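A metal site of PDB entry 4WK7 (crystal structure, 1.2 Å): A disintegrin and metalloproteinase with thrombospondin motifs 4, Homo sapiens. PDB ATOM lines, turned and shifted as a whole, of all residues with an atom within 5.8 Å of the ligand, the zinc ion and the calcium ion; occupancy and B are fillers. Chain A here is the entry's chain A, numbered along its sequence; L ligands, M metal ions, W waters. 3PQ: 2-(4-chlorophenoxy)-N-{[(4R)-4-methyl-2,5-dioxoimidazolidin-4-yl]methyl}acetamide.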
ATOM      1  N   GLN A 107      -3.395 -33.631   5.662  1.00  0.00           N
ATOM      2  CA  GLN A 107      -3.455 -32.241   5.210  1.00  0.00           C
ATOM      3  C   GLN A 107      -2.395 -31.403   5.913  1.00  0.00           C
ATOM      4  O   GLN A 107      -2.225 -31.501   7.128  1.00  0.00           O
ATOM      5  CB  GLN A 107      -4.845 -31.647   5.483  1.00  0.00           C
ATOM      6  CG  GLN A 107      -4.996 -30.150   5.229  1.00  0.00           C
ATOM      7  CD  GLN A 107      -4.911 -29.781   3.756  1.00  0.00           C
ATOM      8  OE1 GLN A 107      -5.608 -30.356   2.922  1.00  0.00           O
ATOM      9  NE2 GLN A 107      -4.054 -28.819   3.442  1.00  0.00           N
ATOM     10  N   ASP A 108      -1.675 -30.591   5.143  1.00  0.00           N
ATOM     11  CA  ASP A 108      -0.750 -29.615   5.690  1.00  0.00           C
ATOM     12  C   ASP A 108      -1.559 -28.486   6.313  1.00  0.00           C
ATOM     13  O   ASP A 108      -2.146 -27.660   5.593  1.00  0.00           O
ATOM     14  CB  ASP A 108       0.192 -29.085   4.599  1.00  0.00           C
ATOM     15  CG  ASP A 108       1.266 -28.155   5.131  1.00  0.00           C
ATOM     16  OD1 ASP A 108       1.322 -27.901   6.360  1.00  0.00           O
ATOM     17  OD2 ASP A 108       2.085 -27.661   4.325  1.00  0.00           O
ATOM     18  N   LEU A 109      -1.616 -28.465   7.635  1.00  0.00           N
ATOM     19  CA  LEU A 109      -2.369 -27.447   8.362  1.00  0.00           C
ATOM     20  C   LEU A 109      -1.572 -26.160   8.461  1.00  0.00           C
ATOM     21  O   LEU A 109      -0.352 -26.190   8.662  1.00  0.00           O
ATOM     22  CB  LEU A 109      -2.719 -27.945   9.771  1.00  0.00           C
ATOM     23  CG  LEU A 109      -3.582 -29.207   9.822  1.00  0.00           C
ATOM     24  CD1 LEU A 109      -3.718 -29.680  11.271  1.00  0.00           C
ATOM     25  CD2 LEU A 109      -4.950 -28.969   9.196  1.00  0.00           C
ATOM     26  N   CYS A 110      -2.257 -25.034   8.329  1.00  0.00           N
ATOM     27  CA  CYS A 110      -1.611 -23.737   8.274  1.00  0.00           C
ATOM     28  C   CYS A 110      -2.287 -22.721   9.187  1.00  0.00           C
ATOM     29  O   CYS A 110      -3.472 -22.859   9.535  1.00  0.00           O
ATOM     30  CB  CYS A 110      -1.594 -23.197   6.842  1.00  0.00           C
ATOM     31  SG  CYS A 110      -1.055 -24.384   5.573  1.00  0.00           S
ATOM     32  N   CYS A 115       2.647 -22.359   7.156  1.00  0.00           N
ATOM     33  CA  CYS A 115       2.086 -23.704   7.327  1.00  0.00           C
ATOM     34  C   CYS A 115       2.925 -24.546   8.294  1.00  0.00           C
ATOM     35  O   CYS A 115       2.868 -25.777   8.252  1.00  0.00           O
ATOM     36  CB  CYS A 115       1.954 -24.388   5.971  1.00  0.00           C
ATOM     37  SG  CYS A 115       0.712 -23.647   4.892  1.00  0.00           S
ATOM     38  N   ASP A 116       3.680 -23.883   9.167  1.00  0.00           N
ATOM     39  CA  ASP A 116       4.539 -24.580  10.121  1.00  0.00           C
ATOM     40  C   ASP A 116       3.759 -25.349  11.183  1.00  0.00           C
ATOM     41  O   ASP A 116       4.257 -26.312  11.759  1.00  0.00           O
ATOM     42  CB  ASP A 116       5.491 -23.596  10.816  1.00  0.00           C
ATOM     43  CG  ASP A 116       6.392 -22.864   9.841  1.00  0.00           C
ATOM     44  OD1 ASP A 116       6.690 -23.421   8.759  1.00  0.00           O
ATOM     45  OD2 ASP A 116       6.818 -21.739  10.170  1.00  0.00           O
ATOM     46  N   THR A 117       2.522 -24.910  11.442  1.00  0.00           N
ATOM     47  CA  THR A 117       1.706 -25.551  12.470  1.00  0.00           C
ATOM     48  C   THR A 117       1.454 -27.019  12.141  1.00  0.00           C
ATOM     49  O   THR A 117       1.340 -27.411  10.980  1.00  0.00           O
ATOM     50  CB  THR A 117       0.368 -24.806  12.730  1.00  0.00           C
ATOM     51  OG1 THR A 117      -0.277 -25.389  13.873  1.00  0.00           O
ATOM     52  CG2 THR A 117      -0.570 -24.880  11.529  1.00  0.00           C
ATOM     53  N   LEU A 118       1.392 -27.830  13.195  1.00  0.00           N
ATOM     54  CA  LEU A 118       1.121 -29.257  13.074  1.00  0.00           C
ATOM     55  C   LEU A 118      -0.192 -29.671  13.744  1.00  0.00           C
ATOM     56  O   LEU A 118      -0.543 -30.845  13.732  1.00  0.00           O
ATOM     57  CB  LEU A 118       2.269 -30.060  13.699  1.00  0.00           C
ATOM     58  CG  LEU A 118       3.609 -29.981  12.962  1.00  0.00           C
ATOM     59  CD1 LEU A 118       4.699 -30.615  13.814  1.00  0.00           C
ATOM     60  CD2 LEU A 118       3.522 -30.663  11.604  1.00  0.00           C
ATOM     61  N   GLY A 119      -0.926 -28.722  14.312  1.00  0.00           N
ATOM     62  CA  GLY A 119      -2.168 -29.077  14.981  1.00  0.00           C
ATOM     63  C   GLY A 119      -2.807 -27.915  15.682  1.00  0.00           C
ATOM     64  O   GLY A 119      -2.244 -26.819  15.741  1.00  0.00           O
ATOM     65  N   MET A 120      -4.006 -28.145  16.200  1.00  0.00           N
ATOM     66  CA  MET A 120      -4.774 -27.114  16.907  1.00  0.00           C
ATOM     67  C   MET A 120      -5.793 -27.776  17.829  1.00  0.00           C
ATOM     68  O   MET A 120      -6.328 -28.824  17.516  1.00  0.00           O
ATOM     69  CB  MET A 120      -5.478 -26.193  15.893  1.00  0.00           C
ATOM     70  CG  MET A 120      -5.983 -24.867  16.455  1.00  0.00           C
ATOM     71  SD  MET A 120      -6.786 -23.755  15.265  1.00  0.00           S
ATOM     72  CE  MET A 120      -5.439 -22.669  14.806  1.00  0.00           C
ATOM     73  N   ALA A 121      -6.073 -27.120  18.958  1.00  0.00           N
ATOM     74  CA  ALA A 121      -7.094 -27.584  19.870  1.00  0.00           C
ATOM     75  C   ALA A 121      -7.663 -26.389  20.602  1.00  0.00           C
ATOM     76  O   ALA A 121      -6.991 -25.372  20.716  1.00  0.00           O
ATOM     77  CB  ALA A 121      -6.500 -28.563  20.875  1.00  0.00           C
ATOM     78  N   GLU A 137      -1.844 -32.794  12.342  1.00  0.00           N
ATOM     79  CA  GLU A 137      -1.225 -33.102  11.060  1.00  0.00           C
ATOM     80  C   GLU A 137      -0.262 -34.268  11.277  1.00  0.00           C
ATOM     81  O   GLU A 137       0.708 -34.131  12.007  1.00  0.00           O
ATOM     82  CB  GLU A 137      -0.453 -31.884  10.544  1.00  0.00           C
ATOM     83  CG  GLU A 137       0.307 -32.146   9.257  1.00  0.00           C
ATOM     84  CD  GLU A 137       1.063 -30.928   8.773  1.00  0.00           C
ATOM     85  OE1 GLU A 137       0.595 -29.789   8.998  1.00  0.00           O
ATOM     86  OE2 GLU A 137       2.136 -31.112   8.156  1.00  0.00           O
ATOM     87  N   PHE A 145       3.675 -36.916  19.767  1.00  0.00           N
ATOM     88  CA  PHE A 145       4.068 -35.703  20.482  1.00  0.00           C
ATOM     89  C   PHE A 145       3.104 -34.555  20.180  1.00  0.00           C
ATOM     90  O   PHE A 145       2.679 -33.841  21.082  1.00  0.00           O
ATOM     91  CB  PHE A 145       5.512 -35.310  20.169  1.00  0.00           C
ATOM     92  CG  PHE A 145       6.530 -36.185  20.852  1.00  0.00           C
ATOM     93  CD1 PHE A 145       6.805 -36.017  22.209  1.00  0.00           C
ATOM     94  CD2 PHE A 145       7.208 -37.171  20.155  1.00  0.00           C
ATOM     95  CE1 PHE A 145       7.730 -36.818  22.852  1.00  0.00           C
ATOM     96  CE2 PHE A 145       8.148 -37.968  20.789  1.00  0.00           C
ATOM     97  CZ  PHE A 145       8.406 -37.803  22.137  1.00  0.00           C
ATOM     98  N   THR A 146       2.748 -34.379  18.907  1.00  0.00           N
ATOM     99  CA  THR A 146       1.761 -33.368  18.555  1.00  0.00           C
ATOM    100  C   THR A 146       0.417 -33.677  19.211  1.00  0.00           C
ATOM    101  O   THR A 146      -0.231 -32.780  19.759  1.00  0.00           O
ATOM    102  CB  THR A 146       1.613 -33.231  17.033  1.00  0.00           C
ATOM    103  OG1 THR A 146       2.904 -32.926  16.486  1.00  0.00           O
ATOM    104  CG2 THR A 146       0.640 -32.112  16.665  1.00  0.00           C
ATOM    105  N   HIS A 149       0.644 -32.649  22.764  1.00  0.00           N
ATOM    106  CA  HIS A 149       0.603 -31.192  22.870  1.00  0.00           C
ATOM    107  C   HIS A 149      -0.828 -30.666  22.766  1.00  0.00           C
ATOM    108  O   HIS A 149      -1.269 -29.849  23.581  1.00  0.00           O
ATOM    109  CB  HIS A 149       1.498 -30.570  21.778  1.00  0.00           C
ATOM    110  CG  HIS A 149       1.531 -29.077  21.791  1.00  0.00           C
ATOM    111  ND1 HIS A 149       2.493 -28.356  22.454  1.00  0.00           N
ATOM    112  CD2 HIS A 149       0.716 -28.158  21.210  1.00  0.00           C
ATOM    113  CE1 HIS A 149       2.270 -27.062  22.294  1.00  0.00           C
ATOM    114  NE2 HIS A 149       1.201 -26.919  21.545  1.00  0.00           N
ATOM    115  N   GLU A 150      -1.559 -31.169  21.775  1.00  0.00           N
ATOM    116  CA  GLU A 150      -2.933 -30.705  21.572  1.00  0.00           C
ATOM    117  C   GLU A 150      -3.847 -31.134  22.715  1.00  0.00           C
ATOM    118  O   GLU A 150      -4.667 -30.352  23.190  1.00  0.00           O
ATOM    119  CB  GLU A 150      -3.490 -31.203  20.224  1.00  0.00           C
ATOM    120  CG  GLU A 150      -2.692 -30.739  19.012  1.00  0.00           C
ATOM    121  CD  GLU A 150      -2.451 -29.245  18.969  1.00  0.00           C
ATOM    122  OE1 GLU A 150      -3.277 -28.472  19.502  1.00  0.00           O
ATOM    123  OE2 GLU A 150      -1.436 -28.837  18.359  1.00  0.00           O
ATOM    124  N   HIS A 153      -3.377 -28.896  25.620  1.00  0.00           N
ATOM    125  CA  HIS A 153      -4.258 -27.734  25.510  1.00  0.00           C
ATOM    126  C   HIS A 153      -5.696 -28.040  25.942  1.00  0.00           C
ATOM    127  O   HIS A 153      -6.304 -27.270  26.677  1.00  0.00           O
ATOM    128  CB  HIS A 153      -4.291 -27.192  24.088  1.00  0.00           C
ATOM    129  CG  HIS A 153      -3.075 -26.405  23.690  1.00  0.00           C
ATOM    130  ND1 HIS A 153      -2.520 -25.432  24.488  1.00  0.00           N
ATOM    131  CD2 HIS A 153      -2.353 -26.425  22.546  1.00  0.00           C
ATOM    132  CE1 HIS A 153      -1.490 -24.887  23.854  1.00  0.00           C
ATOM    133  NE2 HIS A 153      -1.374 -25.476  22.673  1.00  0.00           N
ATOM    134  N   HIS A 159       1.392 -22.634  26.784  1.00  0.00           N
ATOM    135  CA  HIS A 159       2.747 -22.827  26.302  1.00  0.00           C
ATOM    136  C   HIS A 159       3.766 -22.478  27.373  1.00  0.00           C
ATOM    137  O   HIS A 159       3.553 -21.574  28.177  1.00  0.00           O
ATOM    138  CB  HIS A 159       3.029 -21.988  25.068  1.00  0.00           C
ATOM    139  CG  HIS A 159       2.286 -22.450  23.858  1.00  0.00           C
ATOM    140  ND1 HIS A 159       1.852 -21.586  22.882  1.00  0.00           N
ATOM    141  CD2 HIS A 159       1.890 -23.686  23.477  1.00  0.00           C
ATOM    142  CE1 HIS A 159       1.235 -22.269  21.941  1.00  0.00           C
ATOM    143  NE2 HIS A 159       1.232 -23.540  22.280  1.00  0.00           N
ATOM    144  N   HIS A 177      10.008 -29.501  26.690  1.00  0.00           N
ATOM    145  CA  HIS A 177       8.783 -30.141  27.180  1.00  0.00           C
ATOM    146  C   HIS A 177       7.717 -30.192  26.093  1.00  0.00           C
ATOM    147  O   HIS A 177       7.831 -29.527  25.068  1.00  0.00           O
ATOM    148  CB  HIS A 177       8.234 -29.386  28.392  1.00  0.00           C
ATOM    149  CG  HIS A 177       9.244 -29.133  29.462  1.00  0.00           C
ATOM    150  ND1 HIS A 177       9.725 -30.134  30.291  1.00  0.00           N
ATOM    151  CD2 HIS A 177       9.861 -27.997  29.856  1.00  0.00           C
ATOM    152  CE1 HIS A 177      10.595 -29.618  31.135  1.00  0.00           C
ATOM    153  NE2 HIS A 177      10.702 -28.323  30.896  1.00  0.00           N
ATOM    154  N   VAL A 178       6.680 -30.966  26.353  1.00  0.00           N
ATOM    155  CA  VAL A 178       5.584 -31.157  25.394  1.00  0.00           C
ATOM    156  C   VAL A 178       4.874 -29.840  25.050  1.00  0.00           C
ATOM    157  O   VAL A 178       4.496 -29.635  23.907  1.00  0.00           O
ATOM    158  CB  VAL A 178       4.576 -32.207  25.905  1.00  0.00           C
ATOM    159  CG1 VAL A 178       3.308 -32.236  25.041  1.00  0.00           C
ATOM    160  CG2 VAL A 178       5.224 -33.587  25.913  1.00  0.00           C
ATOM    161  N   MET A 179       4.743 -28.943  26.032  1.00  0.00           N
ATOM    162  CA  MET A 179       4.031 -27.693  25.806  1.00  0.00           C
ATOM    163  C   MET A 179       4.929 -26.527  25.391  1.00  0.00           C
ATOM    164  O   MET A 179       4.538 -25.371  25.497  1.00  0.00           O
ATOM    165  CB  MET A 179       3.178 -27.339  27.024  1.00  0.00           C
ATOM    166  CG  MET A 179       2.103 -28.378  27.348  1.00  0.00           C
ATOM    167  SD  MET A 179       1.090 -28.913  25.934  1.00  0.00           S
ATOM    168  CE  MET A 179       0.333 -27.361  25.456  1.00  0.00           C
ATOM    169  N   ALA A 180       6.132 -26.830  24.885  1.00  0.00           N
ATOM    170  CA  ALA A 180       6.874 -25.846  24.110  1.00  0.00           C
ATOM    171  C   ALA A 180       5.988 -25.423  22.929  1.00  0.00           C
ATOM    172  O   ALA A 180       5.180 -26.217  22.455  1.00  0.00           O
ATOM    173  CB  ALA A 180       8.186 -26.432  23.605  1.00  0.00           C
ATOM    174  N   PRO A 181       6.110 -24.168  22.466  1.00  0.00           N
ATOM    175  CA  PRO A 181       5.250 -23.701  21.378  1.00  0.00           C
ATOM    176  C   PRO A 181       5.527 -24.356  20.026  1.00  0.00           C
ATOM    177  O   PRO A 181       4.640 -24.408  19.171  1.00  0.00           O
ATOM    178  CB  PRO A 181       5.529 -22.198  21.323  1.00  0.00           C
ATOM    179  CG  PRO A 181       6.894 -22.052  21.909  1.00  0.00           C
ATOM    180  CD  PRO A 181       7.008 -23.116  22.954  1.00  0.00           C
ATOM    181  N   VAL A 182       6.755 -24.829  19.842  1.00  0.00           N
ATOM    182  CA  VAL A 182       7.139 -25.562  18.639  1.00  0.00           C
ATOM    183  C   VAL A 182       7.824 -26.845  19.068  1.00  0.00           C
ATOM    184  O   VAL A 182       8.445 -26.892  20.128  1.00  0.00           O
ATOM    185  CB  VAL A 182       8.078 -24.730  17.736  1.00  0.00           C
ATOM    186  CG1 VAL A 182       7.394 -23.451  17.283  1.00  0.00           C
ATOM    187  CG2 VAL A 182       9.403 -24.416  18.423  1.00  0.00           C
ATOM    188  N   MET A 183       7.701 -27.877  18.255  1.00  0.00           N
ATOM    189  CA  MET A 183       8.296 -29.167  18.594  1.00  0.00           C
ATOM    190  C   MET A 183       9.816 -29.061  18.693  1.00  0.00           C
ATOM    191  O   MET A 183      10.483 -28.570  17.785  1.00  0.00           O
ATOM    192  CB  MET A 183       7.921 -30.232  17.571  1.00  0.00           C
ATOM    193  CG  MET A 183       8.283 -31.632  18.031  1.00  0.00           C
ATOM    194  SD  MET A 183       7.895 -32.900  16.820  1.00  0.00           S
ATOM    195  CE  MET A 183       6.110 -32.839  16.797  1.00  0.00           C
ATOM    196  N   ALA A 184      10.341 -29.517  19.821  1.00  0.00           N
ATOM    197  CA  ALA A 184      11.781 -29.668  20.023  1.00  0.00           C
ATOM    198  C   ALA A 184      11.980 -30.992  20.744  1.00  0.00           C
ATOM    199  O   ALA A 184      10.999 -31.634  21.148  1.00  0.00           O
ATOM    200  CB  ALA A 184      12.319 -28.528  20.852  1.00  0.00           C
ATOM    201  N   VAL A 186      12.101 -33.555  23.344  1.00  0.00           N
ATOM    202  CA  VAL A 186      11.450 -33.594  24.658  1.00  0.00           C
ATOM    203  C   VAL A 186      12.295 -34.366  25.660  1.00  0.00           C
ATOM    204  O   VAL A 186      12.790 -35.446  25.365  1.00  0.00           O
ATOM    205  CB  VAL A 186      10.037 -34.222  24.541  1.00  0.00           C
ATOM    206  CG1 VAL A 186       9.402 -34.418  25.914  1.00  0.00           C
ATOM    207  CG2 VAL A 186       9.141 -33.341  23.677  1.00  0.00           C
HETATM  208  C7  3PQ L   1       0.931 -23.703  18.687  1.00  0.00           C
HETATM  209  C6  3PQ L   1       0.189 -22.861  16.517  1.00  0.00           C
HETATM  210  N1  3PQ L   1       0.187 -24.563  19.451  1.00  0.00           N
HETATM  211  C5  3PQ L   1       0.702 -24.084  17.255  1.00  0.00           C
HETATM  212  C2  3PQ L   1      -0.555 -25.414  18.699  1.00  0.00           C
HETATM  213  C16 3PQ L   1       4.109 -30.131  18.918  1.00  0.00           C
HETATM  214  C21 3PQ L   1       4.999 -28.425  20.325  1.00  0.00           C
HETATM  215  C17 3PQ L   1       4.797 -31.083  19.655  1.00  0.00           C
HETATM  216  C20 3PQ L   1       5.684 -29.376  21.046  1.00  0.00           C
HETATM  217  C13 3PQ L   1       2.777 -28.217  17.490  1.00  0.00           C
HETATM  218  C9  3PQ L   1       2.015 -24.595  16.679  1.00  0.00           C
HETATM  219  C15 3PQ L   1       4.208 -28.800  19.257  1.00  0.00           C
HETATM  220  C18 3PQ L   1       5.580 -30.702  20.714  1.00  0.00           C
HETATM  221  C11 3PQ L   1       2.148 -27.020  16.813  1.00  0.00           C
HETATM  222  N4  3PQ L   1      -0.307 -25.098  17.392  1.00  0.00           N
HETATM  223  N10 3PQ L   1       2.469 -25.791  17.348  1.00  0.00           N
HETATM  224  O8  3PQ L   1       1.662 -22.814  19.085  1.00  0.00           O
HETATM  225  O3  3PQ L   1      -1.300 -26.283  19.150  1.00  0.00           O
HETATM  226  O12 3PQ L   1       1.411 -27.150  15.857  1.00  0.00           O
HETATM  227  O14 3PQ L   1       3.563 -27.761  18.591  1.00  0.00           O
HETATM  228 CL1  3PQ L   1       6.456 -31.888  21.642  1.00  0.00          CL
HETATM  229 ZN    ZN M   1       0.227 -25.104  21.362  1.00  0.00          ZN
HETATM  230 CA    CA M   2       1.525 -27.636   8.612  1.00  0.00          CA
HETATM  231  O   HOH W   1       3.648 -28.780   8.499  1.00  0.00           O
HETATM  232  O   HOH W   2      -2.490 -24.153  14.944  1.00  0.00           O
HETATM  233  O   HOH W   3       4.458 -26.034  14.721  1.00  0.00           O
HETATM  234  O   HOH W   4       4.419 -22.008  17.465  1.00  0.00           O
HETATM  235  O   HOH W   5      -3.885 -25.247  19.663  1.00  0.00           O
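OE2 of Glu 150 lies close to O3 of the ligand, at 2.7 Å. The backbone NH (N) of Gly 119 lies within hydrogen-bond range of an oxygen (O12) of the ligand (3.2 Å). A nitrogen (N4) of the ligand is in hydrogen-bond range of the backbone carbonyl oxygen of Gly 119 (3.1 Å). O of Pro 181 sits at hydrogen-bond distance from N10 of the ligand (3.2 Å). The backbone NH (N) of Leu 118 lies within hydrogen-bond range of an oxygen (O12) of the ligand (2.7 Å). O12 of the ligand is in hydrogen-bond range of OG1 of Thr 117, at 3.1 Å.
The side-chain carboxylate (OE1) of Glu 150 sits close to the backbone NH (N) of Met 120 (3.4 Å). ND1 of His 149 lies within hydrogen-bond range of O of Val 178 (2.8 Å). O of Leu 118 sits at hydrogen-bond distance from N of Glu 137. A ring nitrogen (ND1) of His 149 lies close to the side-chain sulfur (SD) of Met 179, at 3.8 Å. The side-chain sulfur of Cys 115 forms a disulfide with the side-chain sulfur of Cys 110 (2.0 Å). The side-chain carboxylate of Glu 150 is in hydrogen-bond range of the backbone NH of Ala 121 (3.2 Å). The backbone carbonyl oxygen (O) of Ala 180 sits close to a ring nitrogen (ND1) of His 149 (3.4 Å). The backbone carbonyl oxygen (O) of Gly 119 is in hydrogen-bond range of the side-chain hydroxyl (OG1) of Thr 117 (3.1 Å).
Phe 145 touches the ligand. Thr 146 touches the ligand. O of Val 178 touches C20 of the ligand (3.1 Å). Ala 180 touches the ligand. Val 182 touches the ligand (C to C21, 3.5 Å). Met 183 touches the ligand. CG2 of Val 186 touches CL1 of the ligand, at 3.7 Å. 15 residues have an atom within 4 Å of the ligand: Thr 117, Leu 118, Gly 119, Phe 145, Thr 146, His 149, Glu 150, His 153, His 159, Val 178, Ala 180, Pro 181, Val 182, Met 183 and Val 186.
Within 4 Å of the zinc ion: His 149, His 153 and His 159.
The nearest printed residue that does not touch the calcium ion is Asp 116 (4.1 Å).
The zinc ion is bound by N1 of the ligand (2.0 Å), NE2 of His 149 (2.1 Å), NE2 of His 159 (2.1 Å) and NE2 of His 153 (2.1 Å). The zinc ion has four donor atoms within binding distance.
The calcium ion is bound by OD1 of Asp 108 (2.3 Å), O of Cys 115 (2.3 Å), O of Leu 109 (2.4 Å), OE1 of Glu 137 (2.4 Å), O of Thr 117 (2.4 Å) and water W1 (2.4 Å). The calcium ion has six donor atoms within binding distance.
Water W5 lies within hydrogen-bond range of an oxygen (O3) of the ligand (2.8 Å), the backbone NH of Ala 121 (3.0 Å) and the side-chain carboxylate of Glu 150 (3.3 Å). Water W3 lies within hydrogen-bond range of the backbone carbonyl oxygen of Asp 116 and a nitrogen (N10) of the ligand. Water W4 lies within hydrogen-bond range of the backbone carbonyl oxygen (O) of Pro 181 (3.0 Å) and an oxygen (O8) of the ligand (3.3 Å). Water W2 lies within hydrogen-bond range of the side-chain hydroxyl (OG1) of Thr 117 (2.8 Å), the backbone carbonyl oxygen (O) of Gly 119 (2.8 Å) and a nitrogen (N4) of the ligand (3.4 Å).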
